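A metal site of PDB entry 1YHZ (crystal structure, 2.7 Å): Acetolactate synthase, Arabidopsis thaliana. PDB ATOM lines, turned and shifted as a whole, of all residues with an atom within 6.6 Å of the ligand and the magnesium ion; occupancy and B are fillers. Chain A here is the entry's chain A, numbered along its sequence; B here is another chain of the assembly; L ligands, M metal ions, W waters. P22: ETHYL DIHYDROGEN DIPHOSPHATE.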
ATOM      1  N   GLY A 399     -20.599 -17.209 -13.923  1.00  0.00           N
ATOM      2  CA  GLY A 399     -20.772 -18.056 -12.772  1.00  0.00           C
ATOM      3  C   GLY A 399     -21.189 -17.087 -11.685  1.00  0.00           C
ATOM      4  O   GLY A 399     -21.724 -16.010 -11.984  1.00  0.00           O
ATOM      5  N   VAL A 400     -20.929 -17.428 -10.434  1.00  0.00           N
ATOM      6  CA  VAL A 400     -21.293 -16.546  -9.332  1.00  0.00           C
ATOM      7  C   VAL A 400     -20.052 -16.177  -8.536  1.00  0.00           C
ATOM      8  O   VAL A 400     -19.159 -17.006  -8.355  1.00  0.00           O
ATOM      9  CB  VAL A 400     -22.316 -17.228  -8.395  1.00  0.00           C
ATOM     10  CG1 VAL A 400     -22.580 -16.359  -7.179  1.00  0.00           C
ATOM     11  CG2 VAL A 400     -23.618 -17.498  -9.154  1.00  0.00           C
ATOM     12  N   GLY A 401     -20.004 -14.945  -8.054  1.00  0.00           N
ATOM     13  CA  GLY A 401     -18.859 -14.500  -7.275  1.00  0.00           C
ATOM     14  C   GLY A 401     -18.271 -13.205  -7.776  1.00  0.00           C
ATOM     15  O   GLY A 401     -18.967 -12.375  -8.373  1.00  0.00           O
ATOM     16  N   GLN A 402     -16.971 -13.027  -7.548  1.00  0.00           N
ATOM     17  CA  GLN A 402     -16.287 -11.814  -7.972  1.00  0.00           C
ATOM     18  C   GLN A 402     -16.269 -11.651  -9.490  1.00  0.00           C
ATOM     19  O   GLN A 402     -16.564 -10.565 -10.002  1.00  0.00           O
ATOM     20  CB  GLN A 402     -14.854 -11.790  -7.449  1.00  0.00           C
ATOM     21  CG  GLN A 402     -14.713 -11.891  -5.942  1.00  0.00           C
ATOM     22  CD  GLN A 402     -13.254 -11.870  -5.523  1.00  0.00           C
ATOM     23  OE1 GLN A 402     -12.465 -12.692  -5.969  1.00  0.00           O
ATOM     24  NE2 GLN A 402     -12.903 -10.932  -4.659  1.00  0.00           N
ATOM     25  N   HIS A 403     -15.916 -12.710 -10.203  1.00  0.00           N
ATOM     26  CA  HIS A 403     -15.863 -12.614 -11.661  1.00  0.00           C
ATOM     27  C   HIS A 403     -17.207 -12.159 -12.208  1.00  0.00           C
ATOM     28  O   HIS A 403     -17.276 -11.399 -13.179  1.00  0.00           O
ATOM     29  CB  HIS A 403     -15.459 -13.944 -12.308  1.00  0.00           C
ATOM     30  CG  HIS A 403     -16.503 -15.016 -12.209  1.00  0.00           C
ATOM     31  ND1 HIS A 403     -16.732 -15.731 -11.061  1.00  0.00           N
ATOM     32  CD2 HIS A 403     -17.352 -15.509 -13.142  1.00  0.00           C
ATOM     33  CE1 HIS A 403     -17.674 -16.628 -11.283  1.00  0.00           C
ATOM     34  NE2 HIS A 403     -18.067 -16.518 -12.542  1.00  0.00           N
ATOM     35  N   GLN A 404     -18.280 -12.612 -11.566  1.00  0.00           N
ATOM     36  CA  GLN A 404     -19.627 -12.246 -11.964  1.00  0.00           C
ATOM     37  C   GLN A 404     -19.809 -10.745 -11.802  1.00  0.00           C
ATOM     38  O   GLN A 404     -20.310 -10.074 -12.711  1.00  0.00           O
ATOM     39  CB  GLN A 404     -20.635 -13.018 -11.107  1.00  0.00           C
ATOM     40  CG  GLN A 404     -22.080 -12.603 -11.288  1.00  0.00           C
ATOM     41  CD  GLN A 404     -22.979 -13.353 -10.344  1.00  0.00           C
ATOM     42  OE1 GLN A 404     -22.600 -13.655  -9.208  1.00  0.00           O
ATOM     43  NE2 GLN A 404     -24.190 -13.670 -10.786  1.00  0.00           N
ATOM     44  N   TRP A 406     -17.511  -8.441 -11.726  1.00  0.00           N
ATOM     45  CA  TRP A 406     -16.693  -7.741 -12.698  1.00  0.00           C
ATOM     46  C   TRP A 406     -17.301  -7.823 -14.096  1.00  0.00           C
ATOM     47  O   TRP A 406     -17.312  -6.833 -14.830  1.00  0.00           O
ATOM     48  CB  TRP A 406     -15.258  -8.258 -12.691  1.00  0.00           C
ATOM     49  CG  TRP A 406     -14.526  -7.924 -11.414  1.00  0.00           C
ATOM     50  CD1 TRP A 406     -14.554  -6.730 -10.732  1.00  0.00           C
ATOM     51  CD2 TRP A 406     -13.683  -8.796 -10.657  1.00  0.00           C
ATOM     52  NE1 TRP A 406     -13.785  -6.820  -9.603  1.00  0.00           N
ATOM     53  CE2 TRP A 406     -13.244  -8.071  -9.525  1.00  0.00           C
ATOM     54  CE3 TRP A 406     -13.269 -10.127 -10.820  1.00  0.00           C
ATOM     55  CZ2 TRP A 406     -12.397  -8.637  -8.557  1.00  0.00           C
ATOM     56  CZ3 TRP A 406     -12.432 -10.684  -9.859  1.00  0.00           C
ATOM     57  CH2 TRP A 406     -12.010  -9.943  -8.742  1.00  0.00           C
ATOM     58  N   MET A 428     -23.792 -21.360  -8.477  1.00  0.00           N
ATOM     59  CA  MET A 428     -22.512 -21.604  -9.140  1.00  0.00           C
ATOM     60  C   MET A 428     -22.650 -22.720 -10.180  1.00  0.00           C
ATOM     61  O   MET A 428     -23.518 -23.591 -10.075  1.00  0.00           O
ATOM     62  CB  MET A 428     -21.459 -22.003  -8.092  1.00  0.00           C
ATOM     63  CG  MET A 428     -20.819 -20.818  -7.390  1.00  0.00           C
ATOM     64  SD  MET A 428     -19.733 -21.333  -6.045  1.00  0.00           S
ATOM     65  CE  MET A 428     -18.453 -22.247  -6.946  1.00  0.00           C
ATOM     66  N   ASP A 451     -16.299 -17.202 -16.585  1.00  0.00           N
ATOM     67  CA  ASP A 451     -16.407 -18.051 -15.405  1.00  0.00           C
ATOM     68  C   ASP A 451     -15.319 -17.902 -14.346  1.00  0.00           C
ATOM     69  O   ASP A 451     -14.308 -17.237 -14.557  1.00  0.00           O
ATOM     70  CB  ASP A 451     -16.452 -19.510 -15.848  1.00  0.00           C
ATOM     71  CG  ASP A 451     -17.633 -20.261 -15.281  1.00  0.00           C
ATOM     72  OD1 ASP A 451     -17.954 -20.045 -14.091  1.00  0.00           O
ATOM     73  OD2 ASP A 451     -18.218 -21.082 -16.016  1.00  0.00           O
ATOM     74  N   GLY A 452     -15.549 -18.550 -13.213  1.00  0.00           N
ATOM     75  CA  GLY A 452     -14.602 -18.559 -12.111  1.00  0.00           C
ATOM     76  C   GLY A 452     -14.116 -19.995 -12.028  1.00  0.00           C
ATOM     77  O   GLY A 452     -14.813 -20.905 -12.466  1.00  0.00           O
ATOM     78  N   ASP A 453     -12.931 -20.227 -11.472  1.00  0.00           N
ATOM     79  CA  ASP A 453     -12.403 -21.584 -11.403  1.00  0.00           C
ATOM     80  C   ASP A 453     -13.236 -22.501 -10.526  1.00  0.00           C
ATOM     81  O   ASP A 453     -13.294 -23.695 -10.759  1.00  0.00           O
ATOM     82  CB  ASP A 453     -10.932 -21.587 -10.959  1.00  0.00           C
ATOM     83  CG  ASP A 453     -10.725 -20.942  -9.608  1.00  0.00           C
ATOM     84  OD1 ASP A 453     -11.201 -19.799  -9.407  1.00  0.00           O
ATOM     85  OD2 ASP A 453     -10.080 -21.567  -8.739  1.00  0.00           O
ATOM     86  N   GLY A 454     -13.898 -21.937  -9.526  1.00  0.00           N
ATOM     87  CA  GLY A 454     -14.748 -22.747  -8.670  1.00  0.00           C
ATOM     88  C   GLY A 454     -16.060 -23.096  -9.371  1.00  0.00           C
ATOM     89  O   GLY A 454     -16.472 -24.260  -9.387  1.00  0.00           O
ATOM     90  N   SER A 455     -16.707 -22.084  -9.941  1.00  0.00           N
ATOM     91  CA  SER A 455     -17.977 -22.257 -10.641  1.00  0.00           C
ATOM     92  C   SER A 455     -17.806 -23.104 -11.883  1.00  0.00           C
ATOM     93  O   SER A 455     -18.633 -23.962 -12.174  1.00  0.00           O
ATOM     94  CB  SER A 455     -18.556 -20.901 -11.064  1.00  0.00           C
ATOM     95  OG  SER A 455     -18.730 -20.054  -9.956  1.00  0.00           O
ATOM     96  N   PHE A 456     -16.740 -22.847 -12.618  1.00  0.00           N
ATOM     97  CA  PHE A 456     -16.476 -23.576 -13.852  1.00  0.00           C
ATOM     98  C   PHE A 456     -16.373 -25.079 -13.656  1.00  0.00           C
ATOM     99  O   PHE A 456     -16.930 -25.857 -14.430  1.00  0.00           O
ATOM    100  CB  PHE A 456     -15.202 -23.061 -14.513  1.00  0.00           C
ATOM    101  CG  PHE A 456     -14.842 -23.784 -15.773  1.00  0.00           C
ATOM    102  CD1 PHE A 456     -15.560 -23.560 -16.946  1.00  0.00           C
ATOM    103  CD2 PHE A 456     -13.813 -24.718 -15.796  1.00  0.00           C
ATOM    104  CE1 PHE A 456     -15.257 -24.244 -18.118  1.00  0.00           C
ATOM    105  CE2 PHE A 456     -13.496 -25.422 -16.967  1.00  0.00           C
ATOM    106  CZ  PHE A 456     -14.220 -25.186 -18.134  1.00  0.00           C
ATOM    107  N   LEU A 478     -11.632 -16.700 -15.504  1.00  0.00           N
ATOM    108  CA  LEU A 478     -10.810 -15.864 -14.638  1.00  0.00           C
ATOM    109  C   LEU A 478     -10.394 -16.767 -13.481  1.00  0.00           C
ATOM    110  O   LEU A 478     -11.131 -16.941 -12.513  1.00  0.00           O
ATOM    111  CB  LEU A 478     -11.625 -14.669 -14.132  1.00  0.00           C
ATOM    112  CG  LEU A 478     -12.225 -13.806 -15.263  1.00  0.00           C
ATOM    113  CD1 LEU A 478     -12.776 -12.513 -14.674  1.00  0.00           C
ATOM    114  CD2 LEU A 478     -11.164 -13.510 -16.320  1.00  0.00           C
ATOM    115  N   ASN A 479      -9.201 -17.326 -13.591  1.00  0.00           N
ATOM    116  CA  ASN A 479      -8.681 -18.256 -12.603  1.00  0.00           C
ATOM    117  C   ASN A 479      -7.905 -17.590 -11.454  1.00  0.00           C
ATOM    118  O   ASN A 479      -6.817 -17.056 -11.661  1.00  0.00           O
ATOM    119  CB  ASN A 479      -7.793 -19.268 -13.306  1.00  0.00           C
ATOM    120  CG  ASN A 479      -7.584 -20.514 -12.502  1.00  0.00           C
ATOM    121  OD1 ASN A 479      -7.555 -20.474 -11.262  1.00  0.00           O
ATOM    122  ND2 ASN A 479      -7.404 -21.646 -13.200  1.00  0.00           N
ATOM    123  N   ASN A 480      -8.462 -17.644 -10.245  1.00  0.00           N
ATOM    124  CA  ASN A 480      -7.789 -17.053  -9.095  1.00  0.00           C
ATOM    125  C   ASN A 480      -7.549 -18.074  -7.986  1.00  0.00           C
ATOM    126  O   ASN A 480      -7.243 -17.711  -6.847  1.00  0.00           O
ATOM    127  CB  ASN A 480      -8.588 -15.851  -8.557  1.00  0.00           C
ATOM    128  CG  ASN A 480      -9.871 -16.245  -7.855  1.00  0.00           C
ATOM    129  OD1 ASN A 480     -10.361 -17.366  -7.989  1.00  0.00           O
ATOM    130  ND2 ASN A 480     -10.427 -15.314  -7.097  1.00  0.00           N
ATOM    131  N   GLN A 481      -7.700 -19.356  -8.317  1.00  0.00           N
ATOM    132  CA  GLN A 481      -7.471 -20.454  -7.366  1.00  0.00           C
ATOM    133  C   GLN A 481      -8.290 -20.404  -6.078  1.00  0.00           C
ATOM    134  O   GLN A 481      -8.066 -21.207  -5.180  1.00  0.00           O
ATOM    135  CB  GLN A 481      -5.992 -20.517  -6.999  1.00  0.00           C
ATOM    136  CG  GLN A 481      -5.054 -20.732  -8.166  1.00  0.00           C
ATOM    137  CD  GLN A 481      -5.210 -22.095  -8.806  1.00  0.00           C
ATOM    138  OE1 GLN A 481      -6.168 -22.335  -9.562  1.00  0.00           O
ATOM    139  NE2 GLN A 481      -4.287 -23.001  -8.518  1.00  0.00           N
ATOM    140  N   HIS A 482      -9.234 -19.470  -5.978  1.00  0.00           N
ATOM    141  CA  HIS A 482     -10.040 -19.375  -4.764  1.00  0.00           C
ATOM    142  C   HIS A 482     -11.532 -19.204  -5.018  1.00  0.00           C
ATOM    143  O   HIS A 482     -11.976 -19.068  -6.158  1.00  0.00           O
ATOM    144  CB  HIS A 482      -9.605 -18.172  -3.917  1.00  0.00           C
ATOM    145  CG  HIS A 482      -8.262 -18.313  -3.295  1.00  0.00           C
ATOM    146  ND1 HIS A 482      -7.090 -18.255  -4.017  1.00  0.00           N
ATOM    147  CD2 HIS A 482      -7.897 -18.456  -1.999  1.00  0.00           C
ATOM    148  CE1 HIS A 482      -6.068 -18.358  -3.196  1.00  0.00           C
ATOM    149  NE2 HIS A 482      -6.526 -18.484  -1.958  1.00  0.00           N
ATOM    150  N   LEU A 483     -12.284 -19.237  -3.922  1.00  0.00           N
ATOM    151  CA  LEU A 483     -13.711 -18.992  -3.949  1.00  0.00           C
ATOM    152  C   LEU A 483     -13.707 -17.499  -3.622  1.00  0.00           C
ATOM    153  O   LEU A 483     -13.930 -17.086  -2.474  1.00  0.00           O
ATOM    154  CB  LEU A 483     -14.430 -19.785  -2.860  1.00  0.00           C
ATOM    155  CG  LEU A 483     -14.549 -21.286  -3.124  1.00  0.00           C
ATOM    156  CD1 LEU A 483     -15.233 -21.970  -1.966  1.00  0.00           C
ATOM    157  CD2 LEU A 483     -15.333 -21.523  -4.419  1.00  0.00           C
ATOM    158  N   GLY A 484     -13.393 -16.700  -4.640  1.00  0.00           N
ATOM    159  CA  GLY A 484     -13.295 -15.258  -4.543  1.00  0.00           C
ATOM    160  C   GLY A 484     -14.162 -14.471  -3.575  1.00  0.00           C
ATOM    161  O   GLY A 484     -13.636 -13.853  -2.642  1.00  0.00           O
ATOM    162  N   MET A 485     -15.473 -14.457  -3.815  1.00  0.00           N
ATOM    163  CA  MET A 485     -16.376 -13.688  -2.961  1.00  0.00           C
ATOM    164  C   MET A 485     -16.332 -14.085  -1.486  1.00  0.00           C
ATOM    165  O   MET A 485     -16.374 -13.217  -0.611  1.00  0.00           O
ATOM    166  CB  MET A 485     -17.802 -13.771  -3.479  1.00  0.00           C
ATOM    167  CG  MET A 485     -18.731 -12.761  -2.825  1.00  0.00           C
ATOM    168  SD  MET A 485     -18.181 -11.055  -3.055  1.00  0.00           S
ATOM    169  CE  MET A 485     -18.642 -10.803  -4.757  1.00  0.00           C
ATOM    170  N   VAL A 486     -16.230 -15.383  -1.204  1.00  0.00           N
ATOM    171  CA  VAL A 486     -16.165 -15.810   0.184  1.00  0.00           C
ATOM    172  C   VAL A 486     -14.841 -15.353   0.773  1.00  0.00           C
ATOM    173  O   VAL A 486     -14.763 -14.921   1.923  1.00  0.00           O
ATOM    174  CB  VAL A 486     -16.279 -17.319   0.331  1.00  0.00           C
ATOM    175  CG1 VAL A 486     -16.326 -17.686   1.815  1.00  0.00           C
ATOM    176  CG2 VAL A 486     -17.530 -17.811  -0.373  1.00  0.00           C
ATOM    177  N   LEU A 503      -8.958 -23.292  -3.622  1.00  0.00           N
ATOM    178  CA  LEU A 503      -9.293 -24.378  -4.551  1.00  0.00           C
ATOM    179  C   LEU A 503      -8.108 -25.119  -5.177  1.00  0.00           C
ATOM    180  O   LEU A 503      -8.306 -26.099  -5.889  1.00  0.00           O
ATOM    181  CB  LEU A 503     -10.145 -23.820  -5.688  1.00  0.00           C
ATOM    182  CG  LEU A 503     -11.502 -23.208  -5.333  1.00  0.00           C
ATOM    183  CD1 LEU A 503     -12.058 -22.499  -6.558  1.00  0.00           C
ATOM    184  CD2 LEU A 503     -12.445 -24.285  -4.824  1.00  0.00           C
ATOM    185  N   TYR B  33     -18.914 -27.324   1.883  1.00  0.00           N
ATOM    186  CA  TYR B  33     -18.551 -26.366   0.838  1.00  0.00           C
ATOM    187  C   TYR B  33     -19.057 -25.021   1.335  1.00  0.00           C
ATOM    188  O   TYR B  33     -20.260 -24.823   1.480  1.00  0.00           O
ATOM    189  CB  TYR B  33     -19.225 -26.736  -0.468  1.00  0.00           C
ATOM    190  CG  TYR B  33     -18.636 -26.067  -1.682  1.00  0.00           C
ATOM    191  CD1 TYR B  33     -17.627 -26.684  -2.419  1.00  0.00           C
ATOM    192  CD2 TYR B  33     -19.076 -24.817  -2.092  1.00  0.00           C
ATOM    193  CE1 TYR B  33     -17.077 -26.069  -3.550  1.00  0.00           C
ATOM    194  CE2 TYR B  33     -18.545 -24.190  -3.213  1.00  0.00           C
ATOM    195  CZ  TYR B  33     -17.549 -24.826  -3.943  1.00  0.00           C
ATOM    196  OH  TYR B  33     -17.032 -24.209  -5.058  1.00  0.00           O
ATOM    197  N   PRO B  34     -18.146 -24.075   1.599  1.00  0.00           N
ATOM    198  CA  PRO B  34     -18.472 -22.738   2.090  1.00  0.00           C
ATOM    199  C   PRO B  34     -19.341 -21.867   1.197  1.00  0.00           C
ATOM    200  O   PRO B  34     -19.258 -21.923  -0.030  1.00  0.00           O
ATOM    201  CB  PRO B  34     -17.105 -22.125   2.325  1.00  0.00           C
ATOM    202  CG  PRO B  34     -16.286 -22.737   1.230  1.00  0.00           C
ATOM    203  CD  PRO B  34     -16.706 -24.188   1.306  1.00  0.00           C
HETATM  204  C6  P22 L   1     -17.830 -18.053  -4.678  1.00  0.00           C
HETATM  205  C7  P22 L   1     -17.272 -18.398  -6.100  1.00  0.00           C
HETATM  206  O7  P22 L   1     -16.118 -19.061  -6.654  1.00  0.00           O
HETATM  207  PA  P22 L   1     -15.525 -18.762  -8.132  1.00  0.00           P
HETATM  208  O1A P22 L   1     -14.155 -19.203  -8.194  1.00  0.00           O
HETATM  209  O2A P22 L   1     -16.252 -19.483  -9.132  1.00  0.00           O
HETATM  210  O3A P22 L   1     -15.514 -17.222  -8.493  1.00  0.00           O
HETATM  211  PB  P22 L   1     -14.916 -15.901  -7.858  1.00  0.00           P
HETATM  212  O1B P22 L   1     -15.829 -15.463  -6.795  1.00  0.00           O
HETATM  213  O2B P22 L   1     -14.840 -15.049  -9.022  1.00  0.00           O
HETATM  214  O3B P22 L   1     -13.588 -16.348  -7.406  1.00  0.00           O
HETATM  215 MG    MG M   1     -12.315 -18.197  -8.038  1.00  0.00          MG
HETATM  216  O   HOH W   1     -12.469 -16.965 -10.155  1.00  0.00           O
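Merely in contact with the magnesium ion: Gly 484. Within 4 Å of the magnesium ion: Asp 453, Asn 480, His 482 and Gly 484.
Merely in contact with the ligand: Val 400 (3.3 Å), Gly 401 (3.2 Å), Met 428 (3.8 Å), Gly 452 (3.5 Å) and Leu 483 (3.4 Å). Hydrophobic or aromatic side chains that line the ligand: His 403, Met 428 and Leu 483. The nearest printed residue that does not touch the ligand is Leu 503 (4.2 Å).
Water W1 bridges O of Leu 478 (2.7 Å) and O2B of the ligand (3.3 Å).
The magnesium ion is bound by the backbone carbonyl oxygen of His 482 (2.1 Å), an oxygen (O1A) of the ligand (2.1 Å), the side-chain amide oxygen of Asn 480 (2.1 Å), an oxygen (O3B) of the ligand (2.3 Å), the side-chain carboxylate of Asp 453 (2.4 Å) and water W1 (2.5 Å). The magnesium ion has six donor atoms within binding distance.
O1B of the ligand is in hydrogen-bond range of N of Met 485, at 3.2 Å. N of Gln 402 is in hydrogen-bond range of O1B of the ligand (2.8 Å). An oxygen (O2A) of the ligand lies within hydrogen-bond range of the backbone NH (N) of Ser 455, 2.8 Å away. An oxygen (O1B) of the ligand lies close to the backbone NH of Gly 484. An oxygen (O2A) of the ligand lies within hydrogen-bond range of the side-chain hydroxyl of Ser 455 (2.7 Å). An oxygen (O2B) of the ligand sits at hydrogen-bond distance from the backbone NH of His 403 (2.8 Å). N of Gly 454 is in hydrogen-bond range of O2A of the ligand, at 3.4 Å. ND1 of His 403 sits at hydrogen-bond distance from O2B of the ligand, at 2.9 Å.
NE2 of His 403 lies within hydrogen-bond range of N of Gly 399 (3.0 Å). The side-chain hydroxyl of Ser 455 sits at hydrogen-bond distance from the backbone NH of Val 400 (3.5 Å). N of Gly 452 lies within hydrogen-bond range of NE2 of His 403 (3.3 Å). The side-chain carboxylate of Asp 453 sits close to the backbone NH of Gln 481 (3.3 Å). N of Gly 401 is in hydrogen-bond range of OE1 of Gln 404 (3.1 Å).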
